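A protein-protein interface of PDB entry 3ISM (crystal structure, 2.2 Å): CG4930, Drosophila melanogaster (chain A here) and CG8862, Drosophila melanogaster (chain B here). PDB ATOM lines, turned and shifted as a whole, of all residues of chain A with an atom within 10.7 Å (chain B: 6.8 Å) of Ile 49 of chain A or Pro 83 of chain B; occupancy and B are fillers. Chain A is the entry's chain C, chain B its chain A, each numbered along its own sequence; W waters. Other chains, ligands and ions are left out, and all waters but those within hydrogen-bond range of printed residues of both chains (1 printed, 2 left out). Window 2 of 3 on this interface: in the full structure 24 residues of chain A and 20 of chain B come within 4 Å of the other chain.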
ATOM      1  N   ARG A  43      15.765  -6.045 -27.344  1.00  0.00           N
ATOM      2  CA  ARG A  43      14.777  -4.955 -27.395  1.00  0.00           C
ATOM      3  C   ARG A  43      13.737  -5.000 -26.280  1.00  0.00           C
ATOM      4  O   ARG A  43      13.036  -4.011 -26.029  1.00  0.00           O
ATOM      5  CB  ARG A  43      14.076  -4.924 -28.754  1.00  0.00           C
ATOM      6  CG  ARG A  43      15.036  -4.976 -29.930  1.00  0.00           C
ATOM      7  CD  ARG A  43      14.460  -4.324 -31.166  1.00  0.00           C
ATOM      8  NE  ARG A  43      15.408  -4.356 -32.278  1.00  0.00           N
ATOM      9  CZ  ARG A  43      15.079  -4.131 -33.548  1.00  0.00           C
ATOM     10  NH1 ARG A  43      13.823  -3.853 -33.873  1.00  0.00           N
ATOM     11  NH2 ARG A  43      16.006  -4.181 -34.496  1.00  0.00           N
ATOM     12  N   VAL A  44      13.618  -6.145 -25.621  1.00  0.00           N
ATOM     13  CA  VAL A  44      12.604  -6.294 -24.587  1.00  0.00           C
ATOM     14  C   VAL A  44      13.214  -6.560 -23.206  1.00  0.00           C
ATOM     15  O   VAL A  44      12.916  -5.843 -22.238  1.00  0.00           O
ATOM     16  CB  VAL A  44      11.570  -7.378 -24.959  1.00  0.00           C
ATOM     17  CG1 VAL A  44      10.426  -7.361 -23.976  1.00  0.00           C
ATOM     18  CG2 VAL A  44      11.047  -7.147 -26.364  1.00  0.00           C
ATOM     19  N   GLN A  45      14.067  -7.580 -23.125  1.00  0.00           N
ATOM     20  CA  GLN A  45      14.781  -7.905 -21.889  1.00  0.00           C
ATOM     21  C   GLN A  45      16.015  -7.022 -21.707  1.00  0.00           C
ATOM     22  O   GLN A  45      17.152  -7.506 -21.745  1.00  0.00           O
ATOM     23  CB  GLN A  45      15.201  -9.376 -21.871  1.00  0.00           C
ATOM     24  CG  GLN A  45      14.079 -10.359 -21.632  1.00  0.00           C
ATOM     25  CD  GLN A  45      14.496 -11.802 -21.897  1.00  0.00           C
ATOM     26  OE1 GLN A  45      15.117 -12.111 -22.924  1.00  0.00           O
ATOM     27  NE2 GLN A  45      14.143 -12.697 -20.977  1.00  0.00           N
ATOM     28  N   VAL A  46      15.795  -5.729 -21.498  1.00  0.00           N
ATOM     29  CA  VAL A  46      16.911  -4.813 -21.319  1.00  0.00           C
ATOM     30  C   VAL A  46      17.122  -4.565 -19.831  1.00  0.00           C
ATOM     31  O   VAL A  46      16.226  -4.060 -19.148  1.00  0.00           O
ATOM     32  CB  VAL A  46      16.697  -3.478 -22.081  1.00  0.00           C
ATOM     33  CG1 VAL A  46      17.972  -2.645 -22.063  1.00  0.00           C
ATOM     34  CG2 VAL A  46      16.258  -3.748 -23.517  1.00  0.00           C
ATOM     35  N   ASP A  47      18.303  -4.928 -19.329  1.00  0.00           N
ATOM     36  CA  ASP A  47      18.637  -4.716 -17.920  1.00  0.00           C
ATOM     37  C   ASP A  47      19.117  -3.288 -17.652  1.00  0.00           C
ATOM     38  O   ASP A  47      19.923  -3.047 -16.755  1.00  0.00           O
ATOM     39  CB  ASP A  47      19.672  -5.739 -17.433  1.00  0.00           C
ATOM     40  CG  ASP A  47      19.034  -7.025 -16.917  1.00  0.00           C
ATOM     41  OD1 ASP A  47      17.923  -7.374 -17.380  1.00  0.00           O
ATOM     42  OD2 ASP A  47      19.649  -7.689 -16.052  1.00  0.00           O
ATOM     43  N   GLU A  48      18.621  -2.351 -18.451  1.00  0.00           N
ATOM     44  CA  GLU A  48      18.814  -0.933 -18.219  1.00  0.00           C
ATOM     45  C   GLU A  48      17.421  -0.336 -18.065  1.00  0.00           C
ATOM     46  O   GLU A  48      16.460  -0.855 -18.629  1.00  0.00           O
ATOM     47  CB  GLU A  48      19.535  -0.300 -19.406  1.00  0.00           C
ATOM     48  CG  GLU A  48      20.203   1.023 -19.100  1.00  0.00           C
ATOM     49  CD  GLU A  48      20.194   1.968 -20.285  1.00  0.00           C
ATOM     50  OE1 GLU A  48      20.631   3.128 -20.122  1.00  0.00           O
ATOM     51  OE2 GLU A  48      19.737   1.558 -21.375  1.00  0.00           O
ATOM     52  N   ILE A  49      17.308   0.744 -17.300  1.00  0.00           N
ATOM     53  CA  ILE A  49      16.004   1.368 -17.056  1.00  0.00           C
ATOM     54  C   ILE A  49      15.471   2.069 -18.307  1.00  0.00           C
ATOM     55  O   ILE A  49      16.100   2.986 -18.844  1.00  0.00           O
ATOM     56  CB  ILE A  49      16.011   2.312 -15.826  1.00  0.00           C
ATOM     57  CG1 ILE A  49      16.106   1.486 -14.539  1.00  0.00           C
ATOM     58  CG2 ILE A  49      14.740   3.185 -15.796  1.00  0.00           C
ATOM     59  CD1 ILE A  49      16.317   2.315 -13.295  1.00  0.00           C
ATOM     60  N   VAL A  50      14.312   1.591 -18.755  1.00  0.00           N
ATOM     61  CA  VAL A  50      13.652   2.039 -19.976  1.00  0.00           C
ATOM     62  C   VAL A  50      12.173   2.310 -19.664  1.00  0.00           C
ATOM     63  O   VAL A  50      11.563   1.606 -18.846  1.00  0.00           O
ATOM     64  CB  VAL A  50      13.771   0.955 -21.094  1.00  0.00           C
ATOM     65  CG1 VAL A  50      12.987   1.344 -22.356  1.00  0.00           C
ATOM     66  CG2 VAL A  50      15.250   0.704 -21.453  1.00  0.00           C
ATOM     67  N   ASP A  51      11.612   3.343 -20.287  1.00  0.00           N
ATOM     68  CA  ASP A  51      10.168   3.594 -20.251  1.00  0.00           C
ATOM     69  C   ASP A  51       9.399   2.300 -20.604  1.00  0.00           C
ATOM     70  O   ASP A  51       9.688   1.654 -21.620  1.00  0.00           O
ATOM     71  CB  ASP A  51       9.828   4.716 -21.245  1.00  0.00           C
ATOM     72  CG  ASP A  51       8.357   5.111 -21.231  1.00  0.00           C
ATOM     73  OD1 ASP A  51       7.528   4.418 -20.611  1.00  0.00           O
ATOM     74  OD2 ASP A  51       8.031   6.144 -21.845  1.00  0.00           O
ATOM     75  N   ASP A  52       8.433   1.940 -19.752  1.00  0.00           N
ATOM     76  CA  ASP A  52       7.631   0.731 -19.980  1.00  0.00           C
ATOM     77  C   ASP A  52       6.845   0.820 -21.284  1.00  0.00           C
ATOM     78  O   ASP A  52       6.612  -0.205 -21.913  1.00  0.00           O
ATOM     79  CB  ASP A  52       6.667   0.443 -18.815  1.00  0.00           C
ATOM     80  CG  ASP A  52       7.384   0.225 -17.495  1.00  0.00           C
ATOM     81  OD1 ASP A  52       7.929  -0.874 -17.247  1.00  0.00           O
ATOM     82  OD2 ASP A  52       7.375   1.168 -16.689  1.00  0.00           O
ATOM     83  N   ASP A  53       6.455   2.033 -21.690  1.00  0.00           N
ATOM     84  CA  ASP A  53       5.792   2.264 -22.979  1.00  0.00           C
ATOM     85  C   ASP A  53       6.645   1.769 -24.158  1.00  0.00           C
ATOM     86  O   ASP A  53       6.123   1.165 -25.093  1.00  0.00           O
ATOM     87  CB  ASP A  53       5.447   3.753 -23.173  1.00  0.00           C
ATOM     88  CG  ASP A  53       4.194   4.186 -22.400  1.00  0.00           C
ATOM     89  OD1 ASP A  53       3.380   3.319 -22.020  1.00  0.00           O
ATOM     90  OD2 ASP A  53       4.009   5.411 -22.190  1.00  0.00           O
ATOM     91  N   VAL A  54       7.949   2.037 -24.098  1.00  0.00           N
ATOM     92  CA  VAL A  54       8.900   1.616 -25.133  1.00  0.00           C
ATOM     93  C   VAL A  54       9.009   0.098 -25.170  1.00  0.00           C
ATOM     94  O   VAL A  54       8.940  -0.513 -26.233  1.00  0.00           O
ATOM     95  CB  VAL A  54      10.291   2.248 -24.889  1.00  0.00           C
ATOM     96  CG1 VAL A  54      11.349   1.662 -25.822  1.00  0.00           C
ATOM     97  CG2 VAL A  54      10.217   3.779 -25.042  1.00  0.00           C
ATOM     98  N   THR A  55       9.173  -0.504 -23.996  1.00  0.00           N
ATOM     99  CA  THR A  55       9.321  -1.947 -23.868  1.00  0.00           C
ATOM    100  C   THR A  55       8.068  -2.659 -24.362  1.00  0.00           C
ATOM    101  O   THR A  55       8.161  -3.633 -25.119  1.00  0.00           O
ATOM    102  CB  THR A  55       9.630  -2.341 -22.411  1.00  0.00           C
ATOM    103  OG1 THR A  55      10.817  -1.656 -21.980  1.00  0.00           O
ATOM    104  CG2 THR A  55       9.823  -3.857 -22.273  1.00  0.00           C
ATOM    105  N   ASN A  58       8.013  -2.429 -28.173  1.00  0.00           N
ATOM    106  CA  ASN A  58       9.067  -3.313 -28.678  1.00  0.00           C
ATOM    107  C   ASN A  58       8.620  -4.778 -28.697  1.00  0.00           C
ATOM    108  O   ASN A  58       8.854  -5.504 -29.677  1.00  0.00           O
ATOM    109  CB  ASN A  58      10.354  -3.165 -27.852  1.00  0.00           C
ATOM    110  CG  ASN A  58      11.126  -1.886 -28.178  1.00  0.00           C
ATOM    111  OD1 ASN A  58      10.773  -1.144 -29.105  1.00  0.00           O
ATOM    112  ND2 ASN A  58      12.184  -1.621 -27.407  1.00  0.00           N
ATOM    113  N   GLN B  77       6.737  -0.257 -13.878  1.00  0.00           N
ATOM    114  CA  GLN B  77       7.610   0.298 -12.855  1.00  0.00           C
ATOM    115  C   GLN B  77       7.028   1.592 -12.264  1.00  0.00           C
ATOM    116  O   GLN B  77       6.310   2.349 -12.935  1.00  0.00           O
ATOM    117  CB  GLN B  77       9.020   0.530 -13.390  1.00  0.00           C
ATOM    118  CG  GLN B  77       9.158   1.766 -14.236  1.00  0.00           C
ATOM    119  CD  GLN B  77      10.474   1.798 -14.955  1.00  0.00           C
ATOM    120  OE1 GLN B  77      11.496   2.174 -14.379  1.00  0.00           O
ATOM    121  NE2 GLN B  77      10.469   1.366 -16.216  1.00  0.00           N
ATOM    122  N   ASP B  78       7.321   1.813 -10.996  1.00  0.00           N
ATOM    123  CA  ASP B  78       6.859   2.998 -10.311  1.00  0.00           C
ATOM    124  C   ASP B  78       7.952   4.061 -10.420  1.00  0.00           C
ATOM    125  O   ASP B  78       8.970   3.975  -9.736  1.00  0.00           O
ATOM    126  CB  ASP B  78       6.577   2.642  -8.852  1.00  0.00           C
ATOM    127  CG  ASP B  78       5.914   3.775  -8.079  1.00  0.00           C
ATOM    128  OD1 ASP B  78       5.939   4.943  -8.531  1.00  0.00           O
ATOM    129  OD2 ASP B  78       5.361   3.474  -7.007  1.00  0.00           O
ATOM    130  N   GLU B  79       7.743   5.044 -11.298  1.00  0.00           N
ATOM    131  CA  GLU B  79       8.721   6.109 -11.495  1.00  0.00           C
ATOM    132  C   GLU B  79       8.809   7.078 -10.322  1.00  0.00           C
ATOM    133  O   GLU B  79       9.716   7.891 -10.279  1.00  0.00           O
ATOM    134  CB  GLU B  79       8.472   6.862 -12.809  1.00  0.00           C
ATOM    135  CG  GLU B  79       8.754   5.994 -14.034  1.00  0.00           C
ATOM    136  CD  GLU B  79       8.301   6.613 -15.341  1.00  0.00           C
ATOM    137  OE1 GLU B  79       8.356   7.853 -15.484  1.00  0.00           O
ATOM    138  OE2 GLU B  79       7.898   5.845 -16.246  1.00  0.00           O
ATOM    139  N   ILE B  81       9.490   5.953  -7.405  1.00  0.00           N
ATOM    140  CA  ILE B  81      10.523   5.313  -6.586  1.00  0.00           C
ATOM    141  C   ILE B  81      11.894   5.649  -7.197  1.00  0.00           C
ATOM    142  O   ILE B  81      12.058   5.663  -8.425  1.00  0.00           O
ATOM    143  CB  ILE B  81      10.325   3.775  -6.511  1.00  0.00           C
ATOM    144  CG1 ILE B  81       8.932   3.385  -5.949  1.00  0.00           C
ATOM    145  CG2 ILE B  81      11.467   3.096  -5.727  1.00  0.00           C
ATOM    146  CD1 ILE B  81       8.642   3.817  -4.503  1.00  0.00           C
ATOM    147  N   HIS B  82      12.870   5.956  -6.346  1.00  0.00           N
ATOM    148  CA  HIS B  82      14.234   6.201  -6.821  1.00  0.00           C
ATOM    149  C   HIS B  82      14.729   4.966  -7.612  1.00  0.00           C
ATOM    150  O   HIS B  82      14.487   3.828  -7.187  1.00  0.00           O
ATOM    151  CB  HIS B  82      15.139   6.477  -5.624  1.00  0.00           C
ATOM    152  CG  HIS B  82      16.507   6.950  -5.991  1.00  0.00           C
ATOM    153  ND1 HIS B  82      17.502   6.092  -6.407  1.00  0.00           N
ATOM    154  CD2 HIS B  82      17.050   8.190  -5.999  1.00  0.00           C
ATOM    155  CE1 HIS B  82      18.602   6.783  -6.651  1.00  0.00           C
ATOM    156  NE2 HIS B  82      18.353   8.057  -6.415  1.00  0.00           N
ATOM    157  N   PRO B  83      15.400   5.186  -8.758  1.00  0.00           N
ATOM    158  CA  PRO B  83      15.925   4.104  -9.611  1.00  0.00           C
ATOM    159  C   PRO B  83      16.652   2.971  -8.871  1.00  0.00           C
ATOM    160  O   PRO B  83      16.510   1.813  -9.273  1.00  0.00           O
ATOM    161  CB  PRO B  83      16.921   4.814 -10.547  1.00  0.00           C
ATOM    162  CG  PRO B  83      16.554   6.266 -10.523  1.00  0.00           C
ATOM    163  CD  PRO B  83      15.660   6.528  -9.324  1.00  0.00           C
ATOM    164  N   PHE B  84      17.420   3.284  -7.823  1.00  0.00           N
ATOM    165  CA  PHE B  84      18.162   2.249  -7.094  1.00  0.00           C
ATOM    166  C   PHE B  84      17.237   1.189  -6.455  1.00  0.00           C
ATOM    167  O   PHE B  84      17.670   0.071  -6.214  1.00  0.00           O
ATOM    168  CB  PHE B  84      19.000   2.821  -5.936  1.00  0.00           C
ATOM    169  CG  PHE B  84      20.158   3.722  -6.343  1.00  0.00           C
ATOM    170  CD1 PHE B  84      20.564   3.867  -7.676  1.00  0.00           C
ATOM    171  CD2 PHE B  84      20.874   4.398  -5.346  1.00  0.00           C
ATOM    172  CE1 PHE B  84      21.642   4.693  -8.011  1.00  0.00           C
ATOM    173  CE2 PHE B  84      21.953   5.222  -5.666  1.00  0.00           C
ATOM    174  CZ  PHE B  84      22.339   5.375  -7.011  1.00  0.00           C
ATOM    175  N   PHE B  85      15.990   1.556  -6.146  1.00  0.00           N
ATOM    176  CA  PHE B  85      15.124   0.710  -5.298  1.00  0.00           C
ATOM    177  C   PHE B  85      13.869   0.220  -6.019  1.00  0.00           C
ATOM    178  O   PHE B  85      12.974  -0.388  -5.427  1.00  0.00           O
ATOM    179  CB  PHE B  85      14.742   1.465  -4.022  1.00  0.00           C
ATOM    180  CG  PHE B  85      15.891   2.228  -3.403  1.00  0.00           C
ATOM    181  CD1 PHE B  85      17.072   1.567  -3.033  1.00  0.00           C
ATOM    182  CD2 PHE B  85      15.798   3.589  -3.197  1.00  0.00           C
ATOM    183  CE1 PHE B  85      18.124   2.263  -2.485  1.00  0.00           C
ATOM    184  CE2 PHE B  85      16.853   4.300  -2.627  1.00  0.00           C
ATOM    185  CZ  PHE B  85      18.013   3.634  -2.264  1.00  0.00           C
ATOM    186  N   ARG B  86      13.844   0.444  -7.316  1.00  0.00           N
ATOM    187  CA  ARG B  86      12.696   0.179  -8.134  1.00  0.00           C
ATOM    188  C   ARG B  86      12.759  -1.255  -8.638  1.00  0.00           C
ATOM    189  O   ARG B  86      13.724  -1.629  -9.307  1.00  0.00           O
ATOM    190  CB  ARG B  86      12.776   1.126  -9.320  1.00  0.00           C
ATOM    191  CG  ARG B  86      11.487   1.717  -9.798  1.00  0.00           C
ATOM    192  CD  ARG B  86      11.742   2.546 -11.024  1.00  0.00           C
ATOM    193  NE  ARG B  86      11.957   3.960 -10.717  1.00  0.00           N
ATOM    194  CZ  ARG B  86      12.378   4.856 -11.603  1.00  0.00           C
ATOM    195  NH1 ARG B  86      12.656   4.479 -12.849  1.00  0.00           N
ATOM    196  NH2 ARG B  86      12.522   6.129 -11.246  1.00  0.00           N
ATOM    197  N   SER B  87      11.748  -2.073  -8.350  1.00  0.00           N
ATOM    198  CA  SER B  87      11.690  -3.367  -9.026  1.00  0.00           C
ATOM    199  C   SER B  87      11.256  -3.180 -10.480  1.00  0.00           C
ATOM    200  O   SER B  87      10.617  -2.190 -10.815  1.00  0.00           O
ATOM    201  CB  SER B  87      10.808  -4.379  -8.283  1.00  0.00           C
ATOM    202  OG  SER B  87       9.473  -3.942  -8.144  1.00  0.00           O
ATOM    203  N   GLN B  88      11.654  -4.118 -11.339  1.00  0.00           N
ATOM    204  CA  GLN B  88      11.413  -4.040 -12.776  1.00  0.00           C
ATOM    205  C   GLN B  88      10.862  -5.375 -13.251  1.00  0.00           C
ATOM    206  O   GLN B  88      11.137  -6.401 -12.649  1.00  0.00           O
ATOM    207  CB  GLN B  88      12.716  -3.730 -13.542  1.00  0.00           C
ATOM    208  CG  GLN B  88      13.376  -2.378 -13.211  1.00  0.00           C
ATOM    209  CD  GLN B  88      12.611  -1.158 -13.752  1.00  0.00           C
ATOM    210  OE1 GLN B  88      11.724  -1.274 -14.609  1.00  0.00           O
ATOM    211  NE2 GLN B  88      12.971   0.014 -13.265  1.00  0.00           N
ATOM    212  N   ASN B 182      18.017  -6.195  -9.627  1.00  0.00           N
ATOM    213  CA  ASN B 182      17.612  -5.322  -8.515  1.00  0.00           C
ATOM    214  C   ASN B 182      17.419  -6.030  -7.176  1.00  0.00           C
ATOM    215  O   ASN B 182      16.932  -5.427  -6.213  1.00  0.00           O
ATOM    216  CB  ASN B 182      16.398  -4.481  -8.910  1.00  0.00           C
ATOM    217  CG  ASN B 182      16.693  -3.593 -10.104  1.00  0.00           C
ATOM    218  OD1 ASN B 182      17.676  -2.856 -10.085  1.00  0.00           O
ATOM    219  ND2 ASN B 182      15.889  -3.702 -11.165  1.00  0.00           N
HETATM  220  O   HOH W   1       9.956  -2.838 -15.857  1.00  0.00           O
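NE2 of Gln 77 of chain B sits at hydrogen-bond distance from O of Val 50 of chain A (2.9 Å). The side-chain carboxylate of Asp 52 of chain A lies close to the side-chain amide nitrogen of Gln 77 of chain B (3.1 Å).
OE1 of Gln 77 of chain B sits at hydrogen-bond distance from NH1 of Arg 86 of chain B (3.0 Å). OE1 of Gln 77 of chain B sits at hydrogen-bond distance from NE2 of Gln 88 of chain B, at 2.8 Å. The backbone carbonyl oxygen (O) of Asp 78 of chain B is in hydrogen-bond range of the guanidinium group (NE) of Arg 86 of chain B. The backbone carbonyl oxygen (O) of Glu 79 of chain B lies within hydrogen-bond range of the guanidinium group (NH2) of Arg 86 of chain B (3.5 Å). NE of Arg 86 of chain B is in hydrogen-bond range of O of Ile 81 of chain B (2.9 Å).
Ile 49 of chain A touches Gln 77 of chain B. Ile 49 of chain A touches Pro 83 of chain B. CG2 of Ile 49 of chain A touches NH1 of Arg 86 of chain B, at 3.8 Å. Ile 49 of chain A touches Gln 88 of chain B.
Arg 43 of chain A touches none of the printed residues of chain B. Printed residues of chain B within 4 Å of Ile 49 of chain A: Gln 77, Pro 83, Arg 86 and Gln 88. Printed residues of chain B within 4 Å of Val 50 of chain A: Gln 77. Of the printed residues of chain B, Asp 52 of chain A touches Gln 77 (3.1 Å). Of chain A, only Ile 49 (3.8 Å) comes within 4 Å of Pro 83 of chain B. No residue of chain A comes within 4 Å of Phe 84 of chain B. Arg 86 of chain B touches just one residue of chain A: Ile 49 (3.8 Å). Of the printed residues of chain A, Gln 88 of chain B touches Ile 49. The nearest residue of chain A that does not touch Pro 83 of chain B is Glu 48 of chain A (9.1 Å). The nearest printed residue of chain B that does not touch Val 50 of chain A is Gln 88 of chain B (5.1 Å).
Printed residues of chain A that touch a printed residue of chain B: Ile 49, Val 50 and Asp 52. Hydrophobic or aromatic side chains of chain A within 4 Å of the printed part of chain B: Ile 49. Printed residues of chain B that touch a printed residue of chain A: Gln 77, Pro 83, Arg 86 and Gln 88.
Water W1 bridges OE1 of Gln 88 of chain B (2.7 Å) and OD1 of Asp 52 of chain A (3.1 Å).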
